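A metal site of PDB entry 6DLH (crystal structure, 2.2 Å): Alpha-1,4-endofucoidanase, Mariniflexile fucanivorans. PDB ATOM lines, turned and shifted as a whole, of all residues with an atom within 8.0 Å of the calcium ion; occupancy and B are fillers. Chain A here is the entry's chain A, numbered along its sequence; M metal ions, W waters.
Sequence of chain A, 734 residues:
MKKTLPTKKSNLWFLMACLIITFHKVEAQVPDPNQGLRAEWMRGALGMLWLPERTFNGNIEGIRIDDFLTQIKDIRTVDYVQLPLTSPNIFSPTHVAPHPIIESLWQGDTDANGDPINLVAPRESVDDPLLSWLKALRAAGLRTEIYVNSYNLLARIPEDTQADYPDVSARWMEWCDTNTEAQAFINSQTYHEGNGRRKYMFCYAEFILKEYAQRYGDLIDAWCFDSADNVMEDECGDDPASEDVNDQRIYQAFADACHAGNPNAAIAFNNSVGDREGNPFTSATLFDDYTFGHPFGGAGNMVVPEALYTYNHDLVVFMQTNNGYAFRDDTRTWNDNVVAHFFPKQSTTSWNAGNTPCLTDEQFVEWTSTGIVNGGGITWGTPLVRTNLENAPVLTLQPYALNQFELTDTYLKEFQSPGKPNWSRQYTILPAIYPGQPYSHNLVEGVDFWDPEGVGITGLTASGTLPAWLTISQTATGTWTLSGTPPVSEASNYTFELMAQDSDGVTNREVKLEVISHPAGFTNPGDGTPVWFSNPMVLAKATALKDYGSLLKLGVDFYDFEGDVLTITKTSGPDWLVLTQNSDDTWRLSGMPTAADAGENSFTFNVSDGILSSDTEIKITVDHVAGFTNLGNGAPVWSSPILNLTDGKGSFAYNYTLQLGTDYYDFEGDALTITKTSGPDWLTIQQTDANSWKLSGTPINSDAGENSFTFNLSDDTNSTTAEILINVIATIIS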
ATOM      1  N   GLN A 437      32.833  -8.078 -18.380  1.00  0.00           N
ATOM      2  CA  GLN A 437      31.383  -8.181 -18.260  1.00  0.00           C
ATOM      3  C   GLN A 437      30.980  -9.566 -17.768  1.00  0.00           C
ATOM      4  O   GLN A 437      31.594 -10.563 -18.150  1.00  0.00           O
ATOM      5  CB  GLN A 437      30.702  -7.844 -19.593  1.00  0.00           C
ATOM      6  CG  GLN A 437      30.871  -6.395 -20.020  1.00  0.00           C
ATOM      7  CD  GLN A 437      30.389  -5.421 -18.970  1.00  0.00           C
ATOM      8  OE1 GLN A 437      29.246  -5.474 -18.527  1.00  0.00           O
ATOM      9  NE2 GLN A 437      31.267  -4.519 -18.567  1.00  0.00           N
ATOM     10  N   ASN A 524      32.776   3.849 -27.317  1.00  0.00           N
ATOM     11  CA  ASN A 524      32.244   3.292 -26.075  1.00  0.00           C
ATOM     12  C   ASN A 524      32.123   4.412 -25.051  1.00  0.00           C
ATOM     13  O   ASN A 524      33.113   5.037 -24.691  1.00  0.00           O
ATOM     14  CB  ASN A 524      33.109   2.131 -25.585  1.00  0.00           C
ATOM     15  CG  ASN A 524      32.502   1.348 -24.425  1.00  0.00           C
ATOM     16  OD1 ASN A 524      31.519   1.760 -23.828  1.00  0.00           O
ATOM     17  ND2 ASN A 524      33.101   0.222 -24.100  1.00  0.00           N
ATOM     18  N   PRO A 525      30.902   4.708 -24.534  1.00  0.00           N
ATOM     19  CA  PRO A 525      30.738   5.724 -23.496  1.00  0.00           C
ATOM     20  C   PRO A 525      31.192   5.254 -22.110  1.00  0.00           C
ATOM     21  O   PRO A 525      31.222   6.028 -21.158  1.00  0.00           O
ATOM     22  CB  PRO A 525      29.245   6.052 -23.529  1.00  0.00           C
ATOM     23  CG  PRO A 525      28.588   4.785 -24.072  1.00  0.00           C
ATOM     24  CD  PRO A 525      29.619   4.122 -24.964  1.00  0.00           C
ATOM     25  N   ASP A 527      29.862   3.487 -19.885  1.00  0.00           N
ATOM     26  CA  ASP A 527      28.887   3.353 -18.810  1.00  0.00           C
ATOM     27  C   ASP A 527      27.776   2.347 -19.168  1.00  0.00           C
ATOM     28  O   ASP A 527      26.873   2.115 -18.362  1.00  0.00           O
ATOM     29  CB  ASP A 527      28.338   4.722 -18.384  1.00  0.00           C
ATOM     30  CG  ASP A 527      27.479   5.383 -19.445  1.00  0.00           C
ATOM     31  OD1 ASP A 527      27.437   4.860 -20.577  1.00  0.00           O
ATOM     32  OD2 ASP A 527      26.832   6.396 -19.119  1.00  0.00           O
ATOM     33  N   GLY A 528      27.840   1.780 -20.379  1.00  0.00           N
ATOM     34  CA  GLY A 528      26.880   0.783 -20.818  1.00  0.00           C
ATOM     35  C   GLY A 528      25.750   1.354 -21.682  1.00  0.00           C
ATOM     36  O   GLY A 528      24.889   0.596 -22.136  1.00  0.00           O
ATOM     37  N   THR A 529      25.753   2.666 -21.915  1.00  0.00           N
ATOM     38  CA  THR A 529      24.714   3.331 -22.695  1.00  0.00           C
ATOM     39  C   THR A 529      24.796   2.852 -24.147  1.00  0.00           C
ATOM     40  O   THR A 529      25.880   2.811 -24.739  1.00  0.00           O
ATOM     41  CB  THR A 529      24.826   4.851 -22.595  1.00  0.00           C
ATOM     42  OG1 THR A 529      24.935   5.245 -21.224  1.00  0.00           O
ATOM     43  CG2 THR A 529      23.677   5.598 -23.248  1.00  0.00           C
ATOM     44  N   PRO A 530      23.658   2.447 -24.775  1.00  0.00           N
ATOM     45  CA  PRO A 530      23.636   2.147 -26.205  1.00  0.00           C
ATOM     46  C   PRO A 530      23.651   3.475 -26.959  1.00  0.00           C
ATOM     47  O   PRO A 530      23.026   4.428 -26.510  1.00  0.00           O
ATOM     48  CB  PRO A 530      22.327   1.385 -26.381  1.00  0.00           C
ATOM     49  CG  PRO A 530      21.427   1.957 -25.307  1.00  0.00           C
ATOM     50  CD  PRO A 530      22.352   2.246 -24.131  1.00  0.00           C
ATOM     51  N   VAL A 531      24.381   3.515 -28.090  1.00  0.00           N
ATOM     52  CA  VAL A 531      24.709   4.759 -28.770  1.00  0.00           C
ATOM     53  C   VAL A 531      24.325   4.699 -30.241  1.00  0.00           C
ATOM     54  O   VAL A 531      24.429   3.649 -30.874  1.00  0.00           O
ATOM     55  CB  VAL A 531      26.209   5.107 -28.613  1.00  0.00           C
ATOM     56  CG1 VAL A 531      26.547   5.612 -27.220  1.00  0.00           C
ATOM     57  CG2 VAL A 531      27.106   3.950 -29.012  1.00  0.00           C
ATOM     58  N   TYR A 559      24.546   0.862 -31.655  1.00  0.00           N
ATOM     59  CA  TYR A 559      25.365  -0.213 -31.121  1.00  0.00           C
ATOM     60  C   TYR A 559      25.389  -0.207 -29.601  1.00  0.00           C
ATOM     61  O   TYR A 559      25.128   0.820 -28.973  1.00  0.00           O
ATOM     62  CB  TYR A 559      26.769  -0.171 -31.729  1.00  0.00           C
ATOM     63  CG  TYR A 559      27.653  -1.327 -31.329  1.00  0.00           C
ATOM     64  CD1 TYR A 559      27.457  -2.596 -31.844  1.00  0.00           C
ATOM     65  CD2 TYR A 559      28.689  -1.148 -30.416  1.00  0.00           C
ATOM     66  CE1 TYR A 559      28.265  -3.653 -31.478  1.00  0.00           C
ATOM     67  CE2 TYR A 559      29.498  -2.201 -30.042  1.00  0.00           C
ATOM     68  CZ  TYR A 559      29.284  -3.465 -30.571  1.00  0.00           C
ATOM     69  OH  TYR A 559      30.091  -4.500 -30.196  1.00  0.00           O
ATOM     70  N   ASP A 560      25.721  -1.362 -29.012  1.00  0.00           N
ATOM     71  CA  ASP A 560      25.796  -1.551 -27.572  1.00  0.00           C
ATOM     72  C   ASP A 560      27.042  -2.378 -27.237  1.00  0.00           C
ATOM     73  O   ASP A 560      27.218  -3.484 -27.744  1.00  0.00           O
ATOM     74  CB  ASP A 560      24.535  -2.203 -27.016  1.00  0.00           C
ATOM     75  CG  ASP A 560      24.528  -2.311 -25.501  1.00  0.00           C
ATOM     76  OD1 ASP A 560      25.287  -3.155 -24.947  1.00  0.00           O
ATOM     77  OD2 ASP A 560      23.798  -1.540 -24.870  1.00  0.00           O
ATOM     78  N   PHE A 561      27.877  -1.843 -26.351  1.00  0.00           N
ATOM     79  CA  PHE A 561      29.219  -2.392 -26.178  1.00  0.00           C
ATOM     80  C   PHE A 561      29.197  -3.616 -25.276  1.00  0.00           C
ATOM     81  O   PHE A 561      30.220  -4.298 -25.150  1.00  0.00           O
ATOM     82  CB  PHE A 561      30.218  -1.322 -25.719  1.00  0.00           C
ATOM     83  CG  PHE A 561      30.750  -0.490 -26.856  1.00  0.00           C
ATOM     84  CD1 PHE A 561      30.082   0.656 -27.271  1.00  0.00           C
ATOM     85  CD2 PHE A 561      31.910  -0.868 -27.530  1.00  0.00           C
ATOM     86  CE1 PHE A 561      30.566   1.403 -28.334  1.00  0.00           C
ATOM     87  CE2 PHE A 561      32.387  -0.109 -28.588  1.00  0.00           C
ATOM     88  CZ  PHE A 561      31.716   1.023 -28.982  1.00  0.00           C
ATOM     89  N   GLU A 562      28.034  -3.922 -24.672  1.00  0.00           N
ATOM     90  CA  GLU A 562      27.909  -5.109 -23.833  1.00  0.00           C
ATOM     91  C   GLU A 562      27.055  -6.153 -24.555  1.00  0.00           C
ATOM     92  O   GLU A 562      26.791  -7.210 -23.995  1.00  0.00           O
ATOM     93  CB  GLU A 562      27.330  -4.775 -22.462  1.00  0.00           C
ATOM     94  CG  GLU A 562      28.151  -3.773 -21.672  1.00  0.00           C
ATOM     95  CD  GLU A 562      28.024  -2.338 -22.144  1.00  0.00           C
ATOM     96  OE1 GLU A 562      26.877  -1.903 -22.431  1.00  0.00           O
ATOM     97  OE2 GLU A 562      29.076  -1.658 -22.239  1.00  0.00           O
ATOM     98  N   GLY A 563      26.647  -5.829 -25.786  1.00  0.00           N
ATOM     99  CA  GLY A 563      25.856  -6.722 -26.616  1.00  0.00           C
ATOM    100  C   GLY A 563      24.470  -6.976 -26.049  1.00  0.00           C
ATOM    101  O   GLY A 563      23.886  -8.031 -26.294  1.00  0.00           O
ATOM    102  N   ASP A 564      23.943  -6.001 -25.285  1.00  0.00           N
ATOM    103  CA  ASP A 564      22.595  -6.063 -24.743  1.00  0.00           C
ATOM    104  C   ASP A 564      21.586  -5.951 -25.879  1.00  0.00           C
ATOM    105  O   ASP A 564      21.823  -5.246 -26.852  1.00  0.00           O
ATOM    106  CB  ASP A 564      22.353  -4.970 -23.689  1.00  0.00           C
ATOM    107  CG  ASP A 564      23.263  -5.050 -22.480  1.00  0.00           C
ATOM    108  OD1 ASP A 564      23.605  -6.174 -22.058  1.00  0.00           O
ATOM    109  OD2 ASP A 564      23.637  -3.982 -21.955  1.00  0.00           O
ATOM    110  N   VAL A 565      20.445  -6.643 -25.719  1.00  0.00           N
ATOM    111  CA  VAL A 565      19.316  -6.576 -26.630  1.00  0.00           C
ATOM    112  C   VAL A 565      18.753  -5.152 -26.602  1.00  0.00           C
ATOM    113  O   VAL A 565      18.577  -4.581 -25.529  1.00  0.00           O
ATOM    114  CB  VAL A 565      18.242  -7.639 -26.311  1.00  0.00           C
ATOM    115  CG1 VAL A 565      17.804  -7.630 -24.855  1.00  0.00           C
ATOM    116  CG2 VAL A 565      17.028  -7.558 -27.235  1.00  0.00           C
ATOM    117  N   LEU A 566      18.451  -4.609 -27.786  1.00  0.00           N
ATOM    118  CA  LEU A 566      18.103  -3.195 -27.931  1.00  0.00           C
ATOM    119  C   LEU A 566      16.689  -3.035 -28.477  1.00  0.00           C
ATOM    120  O   LEU A 566      16.218  -3.853 -29.256  1.00  0.00           O
ATOM    121  CB  LEU A 566      19.120  -2.515 -28.857  1.00  0.00           C
ATOM    122  CG  LEU A 566      20.576  -2.579 -28.418  1.00  0.00           C
ATOM    123  CD1 LEU A 566      21.473  -1.846 -29.404  1.00  0.00           C
ATOM    124  CD2 LEU A 566      20.759  -2.021 -27.008  1.00  0.00           C
ATOM    125  N   SER A 608      17.457   1.872 -26.614  1.00  0.00           N
ATOM    126  CA  SER A 608      17.533   1.505 -25.211  1.00  0.00           C
ATOM    127  C   SER A 608      18.022   0.071 -25.055  1.00  0.00           C
ATOM    128  O   SER A 608      17.826  -0.747 -25.948  1.00  0.00           O
ATOM    129  CB  SER A 608      16.198   1.712 -24.537  1.00  0.00           C
ATOM    130  OG  SER A 608      16.146   0.978 -23.320  1.00  0.00           O
ATOM    131  N   ASP A 609      18.663  -0.234 -23.921  1.00  0.00           N
ATOM    132  CA  ASP A 609      19.002  -1.610 -23.595  1.00  0.00           C
ATOM    133  C   ASP A 609      18.155  -2.101 -22.414  1.00  0.00           C
ATOM    134  O   ASP A 609      18.467  -3.114 -21.797  1.00  0.00           O
ATOM    135  CB  ASP A 609      20.512  -1.827 -23.396  1.00  0.00           C
ATOM    136  CG  ASP A 609      21.122  -1.139 -22.179  1.00  0.00           C
ATOM    137  OD1 ASP A 609      20.334  -0.698 -21.294  1.00  0.00           O
ATOM    138  OD2 ASP A 609      22.383  -1.058 -22.120  1.00  0.00           O
ATOM    139  N   GLY A 610      17.078  -1.356 -22.117  1.00  0.00           N
ATOM    140  CA  GLY A 610      16.268  -1.655 -20.960  1.00  0.00           C
ATOM    141  C   GLY A 610      16.706  -0.937 -19.674  1.00  0.00           C
ATOM    142  O   GLY A 610      15.921  -0.864 -18.734  1.00  0.00           O
ATOM    143  N   ILE A 611      17.944  -0.434 -19.619  1.00  0.00           N
ATOM    144  CA  ILE A 611      18.446   0.256 -18.440  1.00  0.00           C
ATOM    145  C   ILE A 611      18.839   1.686 -18.805  1.00  0.00           C
ATOM    146  O   ILE A 611      18.309   2.639 -18.232  1.00  0.00           O
ATOM    147  CB  ILE A 611      19.602  -0.508 -17.763  1.00  0.00           C
ATOM    148  CG1 ILE A 611      19.195  -1.915 -17.304  1.00  0.00           C
ATOM    149  CG2 ILE A 611      20.213   0.305 -16.619  1.00  0.00           C
ATOM    150  CD1 ILE A 611      20.373  -2.830 -16.999  1.00  0.00           C
ATOM    151  N   LEU A 612      19.792   1.831 -19.751  1.00  0.00           N
ATOM    152  CA  LEU A 612      20.220   3.137 -20.240  1.00  0.00           C
ATOM    153  C   LEU A 612      19.799   3.282 -21.700  1.00  0.00           C
ATOM    154  O   LEU A 612      19.554   2.287 -22.384  1.00  0.00           O
ATOM    155  CB  LEU A 612      21.735   3.283 -20.094  1.00  0.00           C
ATOM    156  CG  LEU A 612      22.298   3.092 -18.678  1.00  0.00           C
ATOM    157  CD1 LEU A 612      23.810   2.948 -18.698  1.00  0.00           C
ATOM    158  CD2 LEU A 612      21.873   4.229 -17.768  1.00  0.00           C
ATOM    159  N   SER A 613      19.723   4.542 -22.169  1.00  0.00           N
ATOM    160  CA  SER A 613      19.342   4.862 -23.533  1.00  0.00           C
ATOM    161  C   SER A 613      20.000   6.169 -23.987  1.00  0.00           C
ATOM    162  O   SER A 613      20.679   6.830 -23.206  1.00  0.00           O
ATOM    163  CB  SER A 613      17.848   4.915 -23.671  1.00  0.00           C
ATOM    164  OG  SER A 613      17.312   5.976 -22.904  1.00  0.00           O
HETATM  165 CA    CA M   1      24.569  -1.735 -22.479  1.00  0.00          CA
HETATM  166  O   HOH W   1      24.449  -1.595 -19.909  1.00  0.00           O
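The calcium ion is bound by OE1 of Glu 562, OD2 of Asp 609, O of Gly 528, OD2 of Asp 564, OD2 of Asp 560 and water W1.
Slightly farther from the calcium ion lies the side-chain carboxylate (OD1) of Asp 560 (2.9 Å).
The backbone NH (N) of Leu 612 is in hydrogen-bond range of the side-chain carboxylate (OD1) of Asp 609 (3.0 Å).
N of Ile 611 sits at hydrogen-bond distance from OD1 of Asp 609, 2.9 Å away.
OD1 of Asp 560 lies within hydrogen-bond range of N of Gly 563, 3.1 Å away.
Five residues have an atom within 4 Å of the calcium ion: Gly 528, Asp 560, Glu 562, Asp 564 and Asp 609.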
